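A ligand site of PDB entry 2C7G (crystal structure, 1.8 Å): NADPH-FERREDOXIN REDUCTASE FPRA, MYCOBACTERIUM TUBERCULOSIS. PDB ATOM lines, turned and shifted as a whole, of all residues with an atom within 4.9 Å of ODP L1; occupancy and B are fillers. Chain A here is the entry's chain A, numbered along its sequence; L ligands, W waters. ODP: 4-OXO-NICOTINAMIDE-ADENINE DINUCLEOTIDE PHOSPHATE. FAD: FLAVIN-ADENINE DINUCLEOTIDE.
Water W7 lies within hydrogen-bond range of an oxygen (O3B) of ODP L1 (2.7 Å), the backbone carbonyl oxygen of Gln 204 (2.9 Å) and the backbone NH of Ala 206 (3.4 Å).
Water W4 lies within hydrogen-bond range of O of Ser 321, O1N of ODP L1, N of Gly 156 and N of Ala 159.
Water W14 lies within hydrogen-bond range of N of Tyr 324 and O2N of ODP L1.
Water W12 bridges O2A of ODP L1 (2.9 Å) and O of Pro 364 (3.1 Å).
Water W5 lies within hydrogen-bond range of O2N of ODP L1 (2.9 Å), N of Gly 323 (3.0 Å) and OG of Ser 321 (3.1 Å).
Water W1 lies within hydrogen-bond range of an oxygen (O3X) of ODP L1 (2.9 Å) and the backbone NH of Arg 200 (3.0 Å).
NH2 of Arg 199 is in salt-bridge range of O1X of ODP L1 (2.7 Å).
The backbone NH of Gly 366 lies within hydrogen-bond range of an oxygen (O3D) of ODP L1 (2.8 Å).
NE of Arg 200 is in salt-bridge range of O3X of ODP L1 (2.8 Å).
N of Asn 155 lies within hydrogen-bond range of O3B of ODP L1 (2.9 Å).
The side-chain carboxylate (OE2) of Glu 211 is in hydrogen-bond range of a nitrogen (N7N) of ODP L1, 3.1 Å away.
NH1 of Arg 110 is in hydrogen-bond range of N7A of ODP L1, 3.1 Å away.
O1N of ODP L1 lies within hydrogen-bond range of N of Val 158 (3.1 Å).
O1N of ODP L1 lies within hydrogen-bond range of N of Asn 157 (3.4 Å).
The side-chain amide nitrogen (ND2) of Asn 157 is in hydrogen-bond range of an oxygen (O2D) of ODP L1, 3.2 Å away.
The backbone carbonyl oxygen (O) of Gly 366 lies within hydrogen-bond range of an oxygen (O3') of FAD L2 (3.1 Å).
O2P of FAD L2 lies within hydrogen-bond range of N of Trp 359, at 2.9 Å.
NE1 of Trp 359 lies within hydrogen-bond range of O3' of FAD L2.
Residues that only touch ODP L1: Leu 112 (3.9 Å), Ile 153 (3.7 Å), Gly 156 (3.3 Å), Asp 161 (3.8 Å), Ala 206 (3.6 Å), Ser 321 (3.6 Å), Val 322 (3.3 Å), Gly 323 (3.9 Å), Trp 359 (3.5 Å), Pro 364 (3.5 Å), Thr 365 (3.6 Å) and Val 367 (3.3 Å).
Hydrophobic or aromatic side chains that line ODP L1: Leu 112, Ile 153, Val 158, Ala 206, Val 322, Trp 359 and Val 367.
20 residues have an atom within 4 Å of ODP L1: Arg 110, Leu 112, Ile 153, Asn 155, Gly 156, Asn 157, Val 158, Asp 161, Arg 199, Arg 200, Ala 206, Glu 211, Ser 321, Val 322, Gly 323, Trp 359, Pro 364, Thr 365, Gly 366 and Val 367.
Along chain A the residues within 4 Å of ODP L1 span positions 110 to 367.
N of Ala 206 sits at hydrogen-bond distance from O of Asn 155 (2.8 Å).
OG1 of Thr 208 lies within hydrogen-bond range of OE1 of Glu 211, 2.6 Å away.
The backbone carbonyl oxygen of Val 322 is in hydrogen-bond range of the guanidinium group of Arg 110, 2.8 Å away.
The backbone carbonyl oxygen (O) of Gly 323 is in hydrogen-bond range of the backbone NH (N) of Arg 110, 2.9 Å away.
OD1 of Asn 157 is in hydrogen-bond range of N of Thr 208.
NE1 of Trp 359 lies within hydrogen-bond range of O of Thr 365, 3.0 Å away.
The backbone NH of Ser 321 lies within hydrogen-bond range of the backbone carbonyl oxygen of Ile 153, at 2.8 Å.
The side-chain hydroxyl of Ser 321 sits at hydrogen-bond distance from the backbone NH of Ala 159, at 3.3 Å.
An oxygen (O4) of FAD L2 is in hydrogen-bond range of a nitrogen (N7N) of ODP L1 (3.4 Å).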
ATOM      1  N   ARG A 110      -8.543 -18.304  18.232  1.00  0.00           N
ATOM      2  CA  ARG A 110      -7.472 -18.522  19.192  1.00  0.00           C
ATOM      3  C   ARG A 110      -7.806 -17.821  20.515  1.00  0.00           C
ATOM      4  O   ARG A 110      -8.296 -16.679  20.527  1.00  0.00           O
ATOM      5  CB  ARG A 110      -6.135 -17.987  18.675  1.00  0.00           C
ATOM      6  CG  ARG A 110      -5.586 -18.750  17.467  1.00  0.00           C
ATOM      7  CD  ARG A 110      -4.155 -18.319  17.113  1.00  0.00           C
ATOM      8  NE  ARG A 110      -3.186 -18.808  18.106  1.00  0.00           N
ATOM      9  CZ  ARG A 110      -2.597 -18.052  19.022  1.00  0.00           C
ATOM     10  NH1 ARG A 110      -2.839 -16.746  19.089  1.00  0.00           N
ATOM     11  NH2 ARG A 110      -1.748 -18.604  19.884  1.00  0.00           N
ATOM     12  N   LEU A 112      -6.678 -16.410  24.530  1.00  0.00           N
ATOM     13  CA  LEU A 112      -5.577 -15.769  25.241  1.00  0.00           C
ATOM     14  C   LEU A 112      -5.033 -16.663  26.343  1.00  0.00           C
ATOM     15  O   LEU A 112      -3.847 -16.561  26.700  1.00  0.00           O
ATOM     16  CB  LEU A 112      -6.045 -14.451  25.858  1.00  0.00           C
ATOM     17  CG  LEU A 112      -6.426 -13.339  24.889  1.00  0.00           C
ATOM     18  CD1 LEU A 112      -7.233 -12.302  25.671  1.00  0.00           C
ATOM     19  CD2 LEU A 112      -5.159 -12.745  24.263  1.00  0.00           C
ATOM     20  N   ILE A 153      -7.439  -6.844  21.620  1.00  0.00           N
ATOM     21  CA  ILE A 153      -6.121  -7.465  21.750  1.00  0.00           C
ATOM     22  C   ILE A 153      -5.617  -7.922  20.395  1.00  0.00           C
ATOM     23  O   ILE A 153      -6.331  -8.586  19.654  1.00  0.00           O
ATOM     24  CB  ILE A 153      -6.131  -8.672  22.734  1.00  0.00           C
ATOM     25  CG1 ILE A 153      -6.836  -8.310  24.056  1.00  0.00           C
ATOM     26  CG2 ILE A 153      -4.704  -9.165  22.963  1.00  0.00           C
ATOM     27  CD1 ILE A 153      -6.180  -7.171  24.875  1.00  0.00           C
ATOM     28  N   GLY A 154      -4.393  -7.530  20.043  1.00  0.00           N
ATOM     29  CA  GLY A 154      -3.773  -7.999  18.787  1.00  0.00           C
ATOM     30  C   GLY A 154      -3.373  -6.872  17.847  1.00  0.00           C
ATOM     31  O   GLY A 154      -3.918  -5.771  17.926  1.00  0.00           O
ATOM     32  N   ASN A 155      -2.405  -7.157  16.967  1.00  0.00           N
ATOM     33  CA  ASN A 155      -1.861  -6.186  16.028  1.00  0.00           C
ATOM     34  C   ASN A 155      -1.931  -6.706  14.580  1.00  0.00           C
ATOM     35  O   ASN A 155      -1.007  -6.501  13.791  1.00  0.00           O
ATOM     36  CB  ASN A 155      -0.413  -5.836  16.395  1.00  0.00           C
ATOM     37  CG  ASN A 155      -0.295  -4.676  17.402  1.00  0.00           C
ATOM     38  OD1 ASN A 155       0.819  -4.260  17.695  1.00  0.00           O
ATOM     39  ND2 ASN A 155      -1.426  -4.168  17.921  1.00  0.00           N
ATOM     40  N   GLY A 156      -3.017  -7.386  14.247  1.00  0.00           N
ATOM     41  CA  GLY A 156      -3.278  -7.813  12.881  1.00  0.00           C
ATOM     42  C   GLY A 156      -4.339  -6.925  12.250  1.00  0.00           C
ATOM     43  O   GLY A 156      -4.958  -6.081  12.922  1.00  0.00           O
ATOM     44  N   ASN A 157      -4.583  -7.120  10.954  1.00  0.00           N
ATOM     45  CA  ASN A 157      -5.593  -6.282  10.258  1.00  0.00           C
ATOM     46  C   ASN A 157      -7.027  -6.501  10.771  1.00  0.00           C
ATOM     47  O   ASN A 157      -7.865  -5.632  10.626  1.00  0.00           O
ATOM     48  CB  ASN A 157      -5.565  -6.526   8.761  1.00  0.00           C
ATOM     49  CG  ASN A 157      -4.373  -5.898   8.080  1.00  0.00           C
ATOM     50  OD1 ASN A 157      -3.943  -4.789   8.437  1.00  0.00           O
ATOM     51  ND2 ASN A 157      -3.831  -6.608   7.091  1.00  0.00           N
ATOM     52  N   VAL A 158      -7.290  -7.660  11.361  1.00  0.00           N
ATOM     53  CA  VAL A 158      -8.665  -7.890  11.889  1.00  0.00           C
ATOM     54  C   VAL A 158      -8.879  -6.993  13.108  1.00  0.00           C
ATOM     55  O   VAL A 158      -9.995  -6.521  13.360  1.00  0.00           O
ATOM     56  CB  VAL A 158      -8.934  -9.369  12.202  1.00  0.00           C
ATOM     57  CG1 VAL A 158     -10.340  -9.556  12.800  1.00  0.00           C
ATOM     58  CG2 VAL A 158      -8.824 -10.204  10.923  1.00  0.00           C
ATOM     59  N   ALA A 159      -7.811  -6.743  13.857  1.00  0.00           N
ATOM     60  CA  ALA A 159      -7.902  -5.874  15.027  1.00  0.00           C
ATOM     61  C   ALA A 159      -8.330  -4.485  14.575  1.00  0.00           C
ATOM     62  O   ALA A 159      -9.138  -3.823  15.236  1.00  0.00           O
ATOM     63  CB  ALA A 159      -6.574  -5.841  15.788  1.00  0.00           C
ATOM     64  N   ASP A 161     -10.083  -3.768  11.809  1.00  0.00           N
ATOM     65  CA  ASP A 161     -11.494  -3.864  11.423  1.00  0.00           C
ATOM     66  C   ASP A 161     -12.404  -3.672  12.643  1.00  0.00           C
ATOM     67  O   ASP A 161     -13.375  -2.929  12.592  1.00  0.00           O
ATOM     68  CB  ASP A 161     -11.802  -5.227  10.797  1.00  0.00           C
ATOM     69  CG  ASP A 161     -11.465  -5.289   9.315  1.00  0.00           C
ATOM     70  OD1 ASP A 161     -11.070  -4.241   8.721  1.00  0.00           O
ATOM     71  OD2 ASP A 161     -11.616  -6.385   8.752  1.00  0.00           O
ATOM     72  N   ARG A 199       1.248  -7.083  21.858  1.00  0.00           N
ATOM     73  CA  ARG A 199       2.240  -7.628  22.792  1.00  0.00           C
ATOM     74  C   ARG A 199       3.685  -7.330  22.418  1.00  0.00           C
ATOM     75  O   ARG A 199       4.532  -7.188  23.290  1.00  0.00           O
ATOM     76  CB  ARG A 199       2.080  -9.139  22.961  1.00  0.00           C
ATOM     77  CG  ARG A 199       2.280  -9.989  21.700  1.00  0.00           C
ATOM     78  CD  ARG A 199       2.091 -11.485  22.018  1.00  0.00           C
ATOM     79  NE  ARG A 199       2.200 -12.319  20.836  1.00  0.00           N
ATOM     80  CZ  ARG A 199       2.032 -13.638  20.827  1.00  0.00           C
ATOM     81  NH1 ARG A 199       1.763 -14.285  21.952  1.00  0.00           N
ATOM     82  NH2 ARG A 199       2.129 -14.324  19.689  1.00  0.00           N
ATOM     83  N   ARG A 200       3.979  -7.263  21.118  1.00  0.00           N
ATOM     84  CA  ARG A 200       5.334  -6.914  20.703  1.00  0.00           C
ATOM     85  C   ARG A 200       5.322  -5.439  20.301  1.00  0.00           C
ATOM     86  O   ARG A 200       4.400  -4.711  20.670  1.00  0.00           O
ATOM     87  CB  ARG A 200       5.844  -7.852  19.617  1.00  0.00           C
ATOM     88  CG  ARG A 200       6.023  -9.317  20.135  1.00  0.00           C
ATOM     89  CD  ARG A 200       6.788 -10.210  19.137  1.00  0.00           C
ATOM     90  NE  ARG A 200       6.022 -10.488  17.916  1.00  0.00           N
ATOM     91  CZ  ARG A 200       6.559 -10.839  16.754  1.00  0.00           C
ATOM     92  NH1 ARG A 200       7.886 -10.976  16.649  1.00  0.00           N
ATOM     93  NH2 ARG A 200       5.787 -11.079  15.714  1.00  0.00           N
ATOM     94  N   GLN A 204       7.056  -5.173  14.861  1.00  0.00           N
ATOM     95  CA  GLN A 204       6.553  -6.534  14.779  1.00  0.00           C
ATOM     96  C   GLN A 204       5.069  -6.623  14.381  1.00  0.00           C
ATOM     97  O   GLN A 204       4.521  -7.725  14.257  1.00  0.00           O
ATOM     98  CB  GLN A 204       6.766  -7.253  16.132  1.00  0.00           C
ATOM     99  CG  GLN A 204       8.234  -7.545  16.465  1.00  0.00           C
ATOM    100  CD  GLN A 204       8.991  -6.336  16.988  1.00  0.00           C
ATOM    101  OE1 GLN A 204       8.449  -5.511  17.717  1.00  0.00           O
ATOM    102  NE2 GLN A 204      10.290  -6.272  16.662  1.00  0.00           N
ATOM    103  N   ALA A 206       1.517  -6.905  12.622  1.00  0.00           N
ATOM    104  CA  ALA A 206       1.078  -7.672  11.474  1.00  0.00           C
ATOM    105  C   ALA A 206       0.153  -6.846  10.587  1.00  0.00           C
ATOM    106  O   ALA A 206      -0.297  -7.347   9.549  1.00  0.00           O
ATOM    107  CB  ALA A 206       0.384  -8.976  11.922  1.00  0.00           C
ATOM    108  N   THR A 208      -1.109  -4.148   7.820  1.00  0.00           N
ATOM    109  CA  THR A 208      -0.549  -3.656   6.553  1.00  0.00           C
ATOM    110  C   THR A 208      -0.889  -2.174   6.323  1.00  0.00           C
ATOM    111  O   THR A 208      -1.723  -1.598   7.033  1.00  0.00           O
ATOM    112  CB  THR A 208      -0.872  -4.552   5.341  1.00  0.00           C
ATOM    113  OG1 THR A 208      -2.285  -4.797   5.300  1.00  0.00           O
ATOM    114  CG2 THR A 208      -0.109  -5.882   5.430  1.00  0.00           C
ATOM    115  N   GLU A 211      -4.387  -0.314   5.376  1.00  0.00           N
ATOM    116  CA  GLU A 211      -5.297  -0.538   6.492  1.00  0.00           C
ATOM    117  C   GLU A 211      -5.054   0.417   7.681  1.00  0.00           C
ATOM    118  O   GLU A 211      -6.006   0.880   8.305  1.00  0.00           O
ATOM    119  CB  GLU A 211      -5.212  -2.015   6.915  1.00  0.00           C
ATOM    120  CG  GLU A 211      -5.794  -3.006   5.869  1.00  0.00           C
ATOM    121  CD  GLU A 211      -5.075  -3.023   4.504  1.00  0.00           C
ATOM    122  OE1 GLU A 211      -3.822  -2.900   4.432  1.00  0.00           O
ATOM    123  OE2 GLU A 211      -5.781  -3.178   3.486  1.00  0.00           O
ATOM    124  N   PRO A 275      -2.542  -8.648  27.712  1.00  0.00           N
ATOM    125  CA  PRO A 275      -3.584  -8.744  28.724  1.00  0.00           C
ATOM    126  C   PRO A 275      -3.185  -9.834  29.701  1.00  0.00           C
ATOM    127  O   PRO A 275      -2.752 -10.920  29.279  1.00  0.00           O
ATOM    128  CB  PRO A 275      -4.816  -9.179  27.905  1.00  0.00           C
ATOM    129  CG  PRO A 275      -4.259  -9.937  26.765  1.00  0.00           C
ATOM    130  CD  PRO A 275      -2.947  -9.257  26.429  1.00  0.00           C
ATOM    131  N   SER A 321      -8.434 -10.304  19.218  1.00  0.00           N
ATOM    132  CA  SER A 321      -8.204 -10.503  17.800  1.00  0.00           C
ATOM    133  C   SER A 321      -6.809 -11.084  17.631  1.00  0.00           C
ATOM    134  O   SER A 321      -5.900 -10.482  17.019  1.00  0.00           O
ATOM    135  CB  SER A 321      -8.382  -9.176  17.072  1.00  0.00           C
ATOM    136  OG  SER A 321      -8.470  -9.418  15.690  1.00  0.00           O
ATOM    137  N   VAL A 322      -6.623 -12.275  18.192  1.00  0.00           N
ATOM    138  CA  VAL A 322      -5.312 -12.933  18.189  1.00  0.00           C
ATOM    139  C   VAL A 322      -5.236 -14.145  17.255  1.00  0.00           C
ATOM    140  O   VAL A 322      -4.383 -15.037  17.439  1.00  0.00           O
ATOM    141  CB  VAL A 322      -4.834 -13.267  19.652  1.00  0.00           C
ATOM    142  CG1 VAL A 322      -4.677 -11.950  20.452  1.00  0.00           C
ATOM    143  CG2 VAL A 322      -5.815 -14.243  20.352  1.00  0.00           C
ATOM    144  N   GLY A 323      -6.112 -14.164  16.264  1.00  0.00           N
ATOM    145  CA  GLY A 323      -6.082 -15.148  15.189  1.00  0.00           C
ATOM    146  C   GLY A 323      -7.324 -16.019  15.166  1.00  0.00           C
ATOM    147  O   GLY A 323      -7.872 -16.367  16.225  1.00  0.00           O
ATOM    148  N   TYR A 324      -7.760 -16.354  13.953  1.00  0.00           N
ATOM    149  CA  TYR A 324      -8.746 -17.408  13.737  1.00  0.00           C
ATOM    150  C   TYR A 324      -8.079 -18.779  13.920  1.00  0.00           C
ATOM    151  O   TYR A 324      -6.848 -18.874  14.059  1.00  0.00           O
ATOM    152  CB  TYR A 324      -9.368 -17.243  12.338  1.00  0.00           C
ATOM    153  CG  TYR A 324     -10.405 -16.139  12.238  1.00  0.00           C
ATOM    154  CD1 TYR A 324     -10.109 -14.814  12.612  1.00  0.00           C
ATOM    155  CD2 TYR A 324     -11.686 -16.425  11.756  1.00  0.00           C
ATOM    156  CE1 TYR A 324     -11.090 -13.809  12.515  1.00  0.00           C
ATOM    157  CE2 TYR A 324     -12.662 -15.437  11.659  1.00  0.00           C
ATOM    158  CZ  TYR A 324     -12.363 -14.134  12.024  1.00  0.00           C
ATOM    159  OH  TYR A 324     -13.346 -13.195  11.911  1.00  0.00           O
ATOM    160  N   TRP A 359      -7.194 -21.640   4.108  1.00  0.00           N
ATOM    161  CA  TRP A 359      -6.750 -21.460   5.475  1.00  0.00           C
ATOM    162  C   TRP A 359      -6.729 -22.746   6.281  1.00  0.00           C
ATOM    163  O   TRP A 359      -5.987 -22.847   7.241  1.00  0.00           O
ATOM    164  CB  TRP A 359      -7.624 -20.423   6.163  1.00  0.00           C
ATOM    165  CG  TRP A 359      -7.203 -19.021   5.870  1.00  0.00           C
ATOM    166  CD1 TRP A 359      -6.346 -18.590   4.882  1.00  0.00           C
ATOM    167  CD2 TRP A 359      -7.608 -17.865   6.583  1.00  0.00           C
ATOM    168  NE1 TRP A 359      -6.201 -17.214   4.951  1.00  0.00           N
ATOM    169  CE2 TRP A 359      -6.956 -16.755   6.004  1.00  0.00           C
ATOM    170  CE3 TRP A 359      -8.443 -17.666   7.684  1.00  0.00           C
ATOM    171  CZ2 TRP A 359      -7.126 -15.447   6.477  1.00  0.00           C
ATOM    172  CZ3 TRP A 359      -8.617 -16.359   8.171  1.00  0.00           C
ATOM    173  CH2 TRP A 359      -7.953 -15.268   7.556  1.00  0.00           C
ATOM    174  N   PRO A 364      -4.404 -19.466   9.093  1.00  0.00           N
ATOM    175  CA  PRO A 364      -5.127 -18.218   8.827  1.00  0.00           C
ATOM    176  C   PRO A 364      -4.236 -17.042   8.443  1.00  0.00           C
ATOM    177  O   PRO A 364      -4.165 -16.058   9.185  1.00  0.00           O
ATOM    178  CB  PRO A 364      -5.856 -17.957  10.159  1.00  0.00           C
ATOM    179  CG  PRO A 364      -4.997 -18.581  11.178  1.00  0.00           C
ATOM    180  CD  PRO A 364      -4.375 -19.795  10.529  1.00  0.00           C
ATOM    181  N   THR A 365      -3.595 -17.130   7.277  1.00  0.00           N
ATOM    182  CA  THR A 365      -2.691 -16.080   6.845  1.00  0.00           C
ATOM    183  C   THR A 365      -2.947 -15.693   5.394  1.00  0.00           C
ATOM    184  O   THR A 365      -3.270 -16.513   4.555  1.00  0.00           O
ATOM    185  CB  THR A 365      -1.206 -16.496   7.019  1.00  0.00           C
ATOM    186  OG1 THR A 365      -0.918 -17.627   6.187  1.00  0.00           O
ATOM    187  CG2 THR A 365      -0.928 -16.890   8.461  1.00  0.00           C
ATOM    188  N   GLY A 366      -2.793 -14.415   5.106  1.00  0.00           N
ATOM    189  CA  GLY A 366      -2.853 -13.948   3.722  1.00  0.00           C
ATOM    190  C   GLY A 366      -4.178 -13.338   3.322  1.00  0.00           C
ATOM    191  O   GLY A 366      -5.252 -13.633   3.877  1.00  0.00           O
ATOM    192  N   VAL A 367      -4.082 -12.490   2.311  1.00  0.00           N
ATOM    193  CA  VAL A 367      -5.235 -11.841   1.728  1.00  0.00           C
ATOM    194  C   VAL A 367      -6.003 -12.820   0.829  1.00  0.00           C
ATOM    195  O   VAL A 367      -5.556 -13.941   0.563  1.00  0.00           O
ATOM    196  CB  VAL A 367      -4.778 -10.612   0.921  1.00  0.00           C
ATOM    197  CG1 VAL A 367      -4.138  -9.625   1.858  1.00  0.00           C
ATOM    198  CG2 VAL A 367      -3.793 -11.018  -0.206  1.00  0.00           C
HETATM  199  O1X ODP L   1       2.304 -12.998  17.291  1.00  0.00           O
HETATM  200  P2B ODP L   1       2.478 -11.514  17.249  1.00  0.00           P
HETATM  201  O2X ODP L   1       2.895 -11.035  15.901  1.00  0.00           O
HETATM  202  O3X ODP L   1       3.266 -10.961  18.413  1.00  0.00           O
HETATM  203  O2B ODP L   1       1.021 -10.888  17.524  1.00  0.00           O
HETATM  204  C2B ODP L   1      -0.150 -11.426  16.917  1.00  0.00           C
HETATM  205  C3B ODP L   1      -0.699 -10.562  15.788  1.00  0.00           C
HETATM  206  O3B ODP L   1      -0.504  -9.179  16.080  1.00  0.00           O
HETATM  207  C1B ODP L   1      -1.291 -11.313  17.889  1.00  0.00           C
HETATM  208  N9A ODP L   1      -1.335 -12.347  18.951  1.00  0.00           N
HETATM  209  C8A ODP L   1      -1.343 -13.680  18.808  1.00  0.00           C
HETATM  210  N7A ODP L   1      -1.408 -14.224  20.058  1.00  0.00           N
HETATM  211  C5A ODP L   1      -1.441 -13.214  20.958  1.00  0.00           C
HETATM  212  C4A ODP L   1      -1.387 -12.016  20.244  1.00  0.00           C
HETATM  213  N3A ODP L   1      -1.405 -10.823  20.896  1.00  0.00           N
HETATM  214  C2A ODP L   1      -1.484 -10.805  22.247  1.00  0.00           C
HETATM  215  N1A ODP L   1      -1.536 -11.948  22.960  1.00  0.00           N
HETATM  216  C6A ODP L   1      -1.513 -13.154  22.353  1.00  0.00           C
HETATM  217  N6A ODP L   1      -1.555 -14.309  23.097  1.00  0.00           N
HETATM  218  O4B ODP L   1      -2.466 -11.425  17.088  1.00  0.00           O
HETATM  219  C4B ODP L   1      -2.203 -10.821  15.822  1.00  0.00           C
HETATM  220  C5B ODP L   1      -2.652 -11.765  14.724  1.00  0.00           C
HETATM  221  O5B ODP L   1      -2.494 -11.069  13.498  1.00  0.00           O
HETATM  222  PA  ODP L   1      -2.723 -11.844  12.113  1.00  0.00           P
HETATM  223  O1A ODP L   1      -2.500 -10.840  10.988  1.00  0.00           O
HETATM  224  O2A ODP L   1      -1.950 -13.131  12.099  1.00  0.00           O
HETATM  225  O3  ODP L   1      -4.265 -12.336  12.212  1.00  0.00           O
HETATM  226  PN  ODP L   1      -5.643 -11.539  11.857  1.00  0.00           P
HETATM  227  O1N ODP L   1      -5.595 -10.077  12.212  1.00  0.00           O
HETATM  228  O2N ODP L   1      -6.703 -12.444  12.416  1.00  0.00           O
HETATM  229  O5D ODP L   1      -5.773 -11.637  10.257  1.00  0.00           O
HETATM  230  C5D ODP L   1      -5.718 -12.910   9.584  1.00  0.00           C
HETATM  231  C4D ODP L   1      -5.223 -12.793   8.141  1.00  0.00           C
HETATM  232  O4D ODP L   1      -6.252 -12.186   7.337  1.00  0.00           O
HETATM  233  C1D ODP L   1      -5.731 -11.009   6.683  1.00  0.00           C
HETATM  234  C2D ODP L   1      -4.551 -10.602   7.573  1.00  0.00           C
HETATM  235  O2D ODP L   1      -3.617  -9.752   6.888  1.00  0.00           O
HETATM  236  C3D ODP L   1      -3.972 -11.914   8.049  1.00  0.00           C
HETATM  237  O3D ODP L   1      -3.100 -12.497   7.074  1.00  0.00           O
HETATM  238  N1N ODP L   1      -6.576  -9.819   6.634  1.00  0.00           N
HETATM  239  C2N ODP L   1      -6.304  -8.930   5.658  1.00  0.00           C
HETATM  240  C3N ODP L   1      -7.004  -7.737   5.525  1.00  0.00           C
HETATM  241  C7N ODP L   1      -6.632  -6.838   4.379  1.00  0.00           C
HETATM  242  N7N ODP L   1      -7.257  -5.780   4.104  1.00  0.00           N
HETATM  243  O7N ODP L   1      -5.588  -7.202   3.645  1.00  0.00           O
HETATM  244  C4N ODP L   1      -7.992  -7.447   6.452  1.00  0.00           C
HETATM  245  O99 ODP L   1      -8.633  -6.369   6.419  1.00  0.00           O
HETATM  246  C5N ODP L   1      -8.249  -8.371   7.488  1.00  0.00           C
HETATM  247  C6N ODP L   1      -7.519  -9.555   7.563  1.00  0.00           C
HETATM  248  PA  FAD L   2     -13.319 -19.083   4.172  1.00  0.00           P
HETATM  249  O1A FAD L   2     -13.390 -19.011   5.680  1.00  0.00           O
HETATM  250  O2A FAD L   2     -13.419 -17.788   3.389  1.00  0.00           O
HETATM  251  O5B FAD L   2     -14.422 -20.088   3.602  1.00  0.00           O
HETATM  252  C5B FAD L   2     -14.615 -21.351   4.222  1.00  0.00           C
HETATM  253  C4B FAD L   2     -16.045 -21.836   3.910  1.00  0.00           C
HETATM  254  O4B FAD L   2     -16.157 -23.172   4.382  1.00  0.00           O
HETATM  255  C3B FAD L   2     -17.105 -21.031   4.671  1.00  0.00           C
HETATM  256  O3B FAD L   2     -18.133 -20.598   3.779  1.00  0.00           O
HETATM  257  C2B FAD L   2     -17.646 -22.024   5.697  1.00  0.00           C
HETATM  258  O2B FAD L   2     -19.015 -21.826   6.042  1.00  0.00           O
HETATM  259  C1B FAD L   2     -17.410 -23.358   4.995  1.00  0.00           C
HETATM  260  N9A FAD L   2     -17.301 -24.509   5.910  1.00  0.00           N
HETATM  261  C8A FAD L   2     -16.546 -24.611   7.051  1.00  0.00           C
HETATM  262  N7A FAD L   2     -16.747 -25.841   7.577  1.00  0.00           N
HETATM  263  C5A FAD L   2     -17.624 -26.519   6.794  1.00  0.00           C
HETATM  264  C6A FAD L   2     -18.177 -27.799   6.877  1.00  0.00           C
HETATM  265  N6A FAD L   2     -17.807 -28.622   7.856  1.00  0.00           N
HETATM  266  N1A FAD L   2     -19.052 -28.241   5.909  1.00  0.00           N
HETATM  267  C2A FAD L   2     -19.397 -27.391   4.874  1.00  0.00           C
HETATM  268  N3A FAD L   2     -18.853 -26.119   4.809  1.00  0.00           N
HETATM  269  C4A FAD L   2     -17.975 -25.693   5.740  1.00  0.00           C
HETATM  270  N1  FAD L   2      -8.587 -10.512   2.761  1.00  0.00           N
HETATM  271  C2  FAD L   2      -8.460  -9.483   1.856  1.00  0.00           C
HETATM  272  O2  FAD L   2      -7.816  -9.672   0.819  1.00  0.00           O
HETATM  273  N3  FAD L   2      -9.071  -8.271   2.130  1.00  0.00           N
HETATM  274  C4  FAD L   2      -9.814  -8.083   3.294  1.00  0.00           C
HETATM  275  O4  FAD L   2     -10.353  -6.994   3.514  1.00  0.00           O
HETATM  276  C4X FAD L   2      -9.953  -9.133   4.215  1.00  0.00           C
HETATM  277  N5  FAD L   2     -10.682  -8.966   5.380  1.00  0.00           N
HETATM  278  C5X FAD L   2     -10.792 -10.038   6.278  1.00  0.00           C
HETATM  279  C6  FAD L   2     -11.511  -9.886   7.466  1.00  0.00           C
HETATM  280  C7  FAD L   2     -11.625 -10.947   8.356  1.00  0.00           C
HETATM  281  C7M FAD L   2     -12.332 -10.693   9.679  1.00  0.00           C
HETATM  282  C8  FAD L   2     -10.988 -12.158   8.068  1.00  0.00           C
HETATM  283  C8M FAD L   2     -10.892 -13.263   9.073  1.00  0.00           C
HETATM  284  C9  FAD L   2     -10.254 -12.313   6.905  1.00  0.00           C
HETATM  285  C9A FAD L   2     -10.154 -11.248   5.989  1.00  0.00           C
HETATM  286  N10 FAD L   2      -9.425 -11.398   4.811  1.00  0.00           N
HETATM  287  C10 FAD L   2      -9.325 -10.340   3.924  1.00  0.00           C
HETATM  288  C1' FAD L   2      -8.740 -12.694   4.445  1.00  0.00           C
HETATM  289  C2' FAD L   2      -9.667 -13.634   3.675  1.00  0.00           C
HETATM  290  O2' FAD L   2     -10.952 -13.590   4.278  1.00  0.00           O
HETATM  291  C3' FAD L   2      -9.105 -15.066   3.627  1.00  0.00           C
HETATM  292  O3' FAD L   2      -7.862 -15.058   2.966  1.00  0.00           O
HETATM  293  C4' FAD L   2     -10.022 -16.047   2.884  1.00  0.00           C
HETATM  294  O4' FAD L   2     -11.399 -15.798   3.122  1.00  0.00           O
HETATM  295  C5' FAD L   2      -9.702 -17.499   3.252  1.00  0.00           C
HETATM  296  O5' FAD L   2     -10.470 -18.275   2.348  1.00  0.00           O
HETATM  297  P   FAD L   2     -10.864 -19.792   2.694  1.00  0.00           P
HETATM  298  O1P FAD L   2     -11.494 -20.333   1.451  1.00  0.00           O
HETATM  299  O2P FAD L   2      -9.697 -20.598   3.165  1.00  0.00           O
HETATM  300  O3P FAD L   2     -11.889 -19.777   3.932  1.00  0.00           O
HETATM  301  O   HOH W   1       2.386  -8.168  18.713  1.00  0.00           O
HETATM  302  O   HOH W   2      -0.414  -8.387  19.717  1.00  0.00           O
HETATM  303  O   HOH W   3       0.251 -13.840  13.232  1.00  0.00           O
HETATM  304  O   HOH W   4      -5.693  -9.014  14.790  1.00  0.00           O
HETATM  305  O   HOH W   5      -8.161 -12.378  14.907  1.00  0.00           O
HETATM  306  O   HOH W   6      -0.366 -11.834   9.494  1.00  0.00           O
HETATM  307  O   HOH W   7       2.028  -8.456  15.570  1.00  0.00           O
HETATM  308  O   HOH W   8      -2.928  -7.143   3.825  1.00  0.00           O
HETATM  309  O   HOH W   9       2.530 -11.861  13.492  1.00  0.00           O
HETATM  310  O   HOH W  10      -0.778 -11.193   7.005  1.00  0.00           O
HETATM  311  O   HOH W  11      -0.251 -11.661  25.394  1.00  0.00           O
HETATM  312  O   HOH W  12      -3.587 -15.477  12.175  1.00  0.00           O
HETATM  313  O   HOH W  13      -2.715  -8.832   9.554  1.00  0.00           O
HETATM  314  O   HOH W  14      -6.221 -15.166  11.995  1.00  0.00           O
HETATM  315  O   HOH W  15       0.638 -14.778  15.707  1.00  0.00           O
HETATM  316  O   HOH W  16      -1.856  -9.445   4.828  1.00  0.00           O
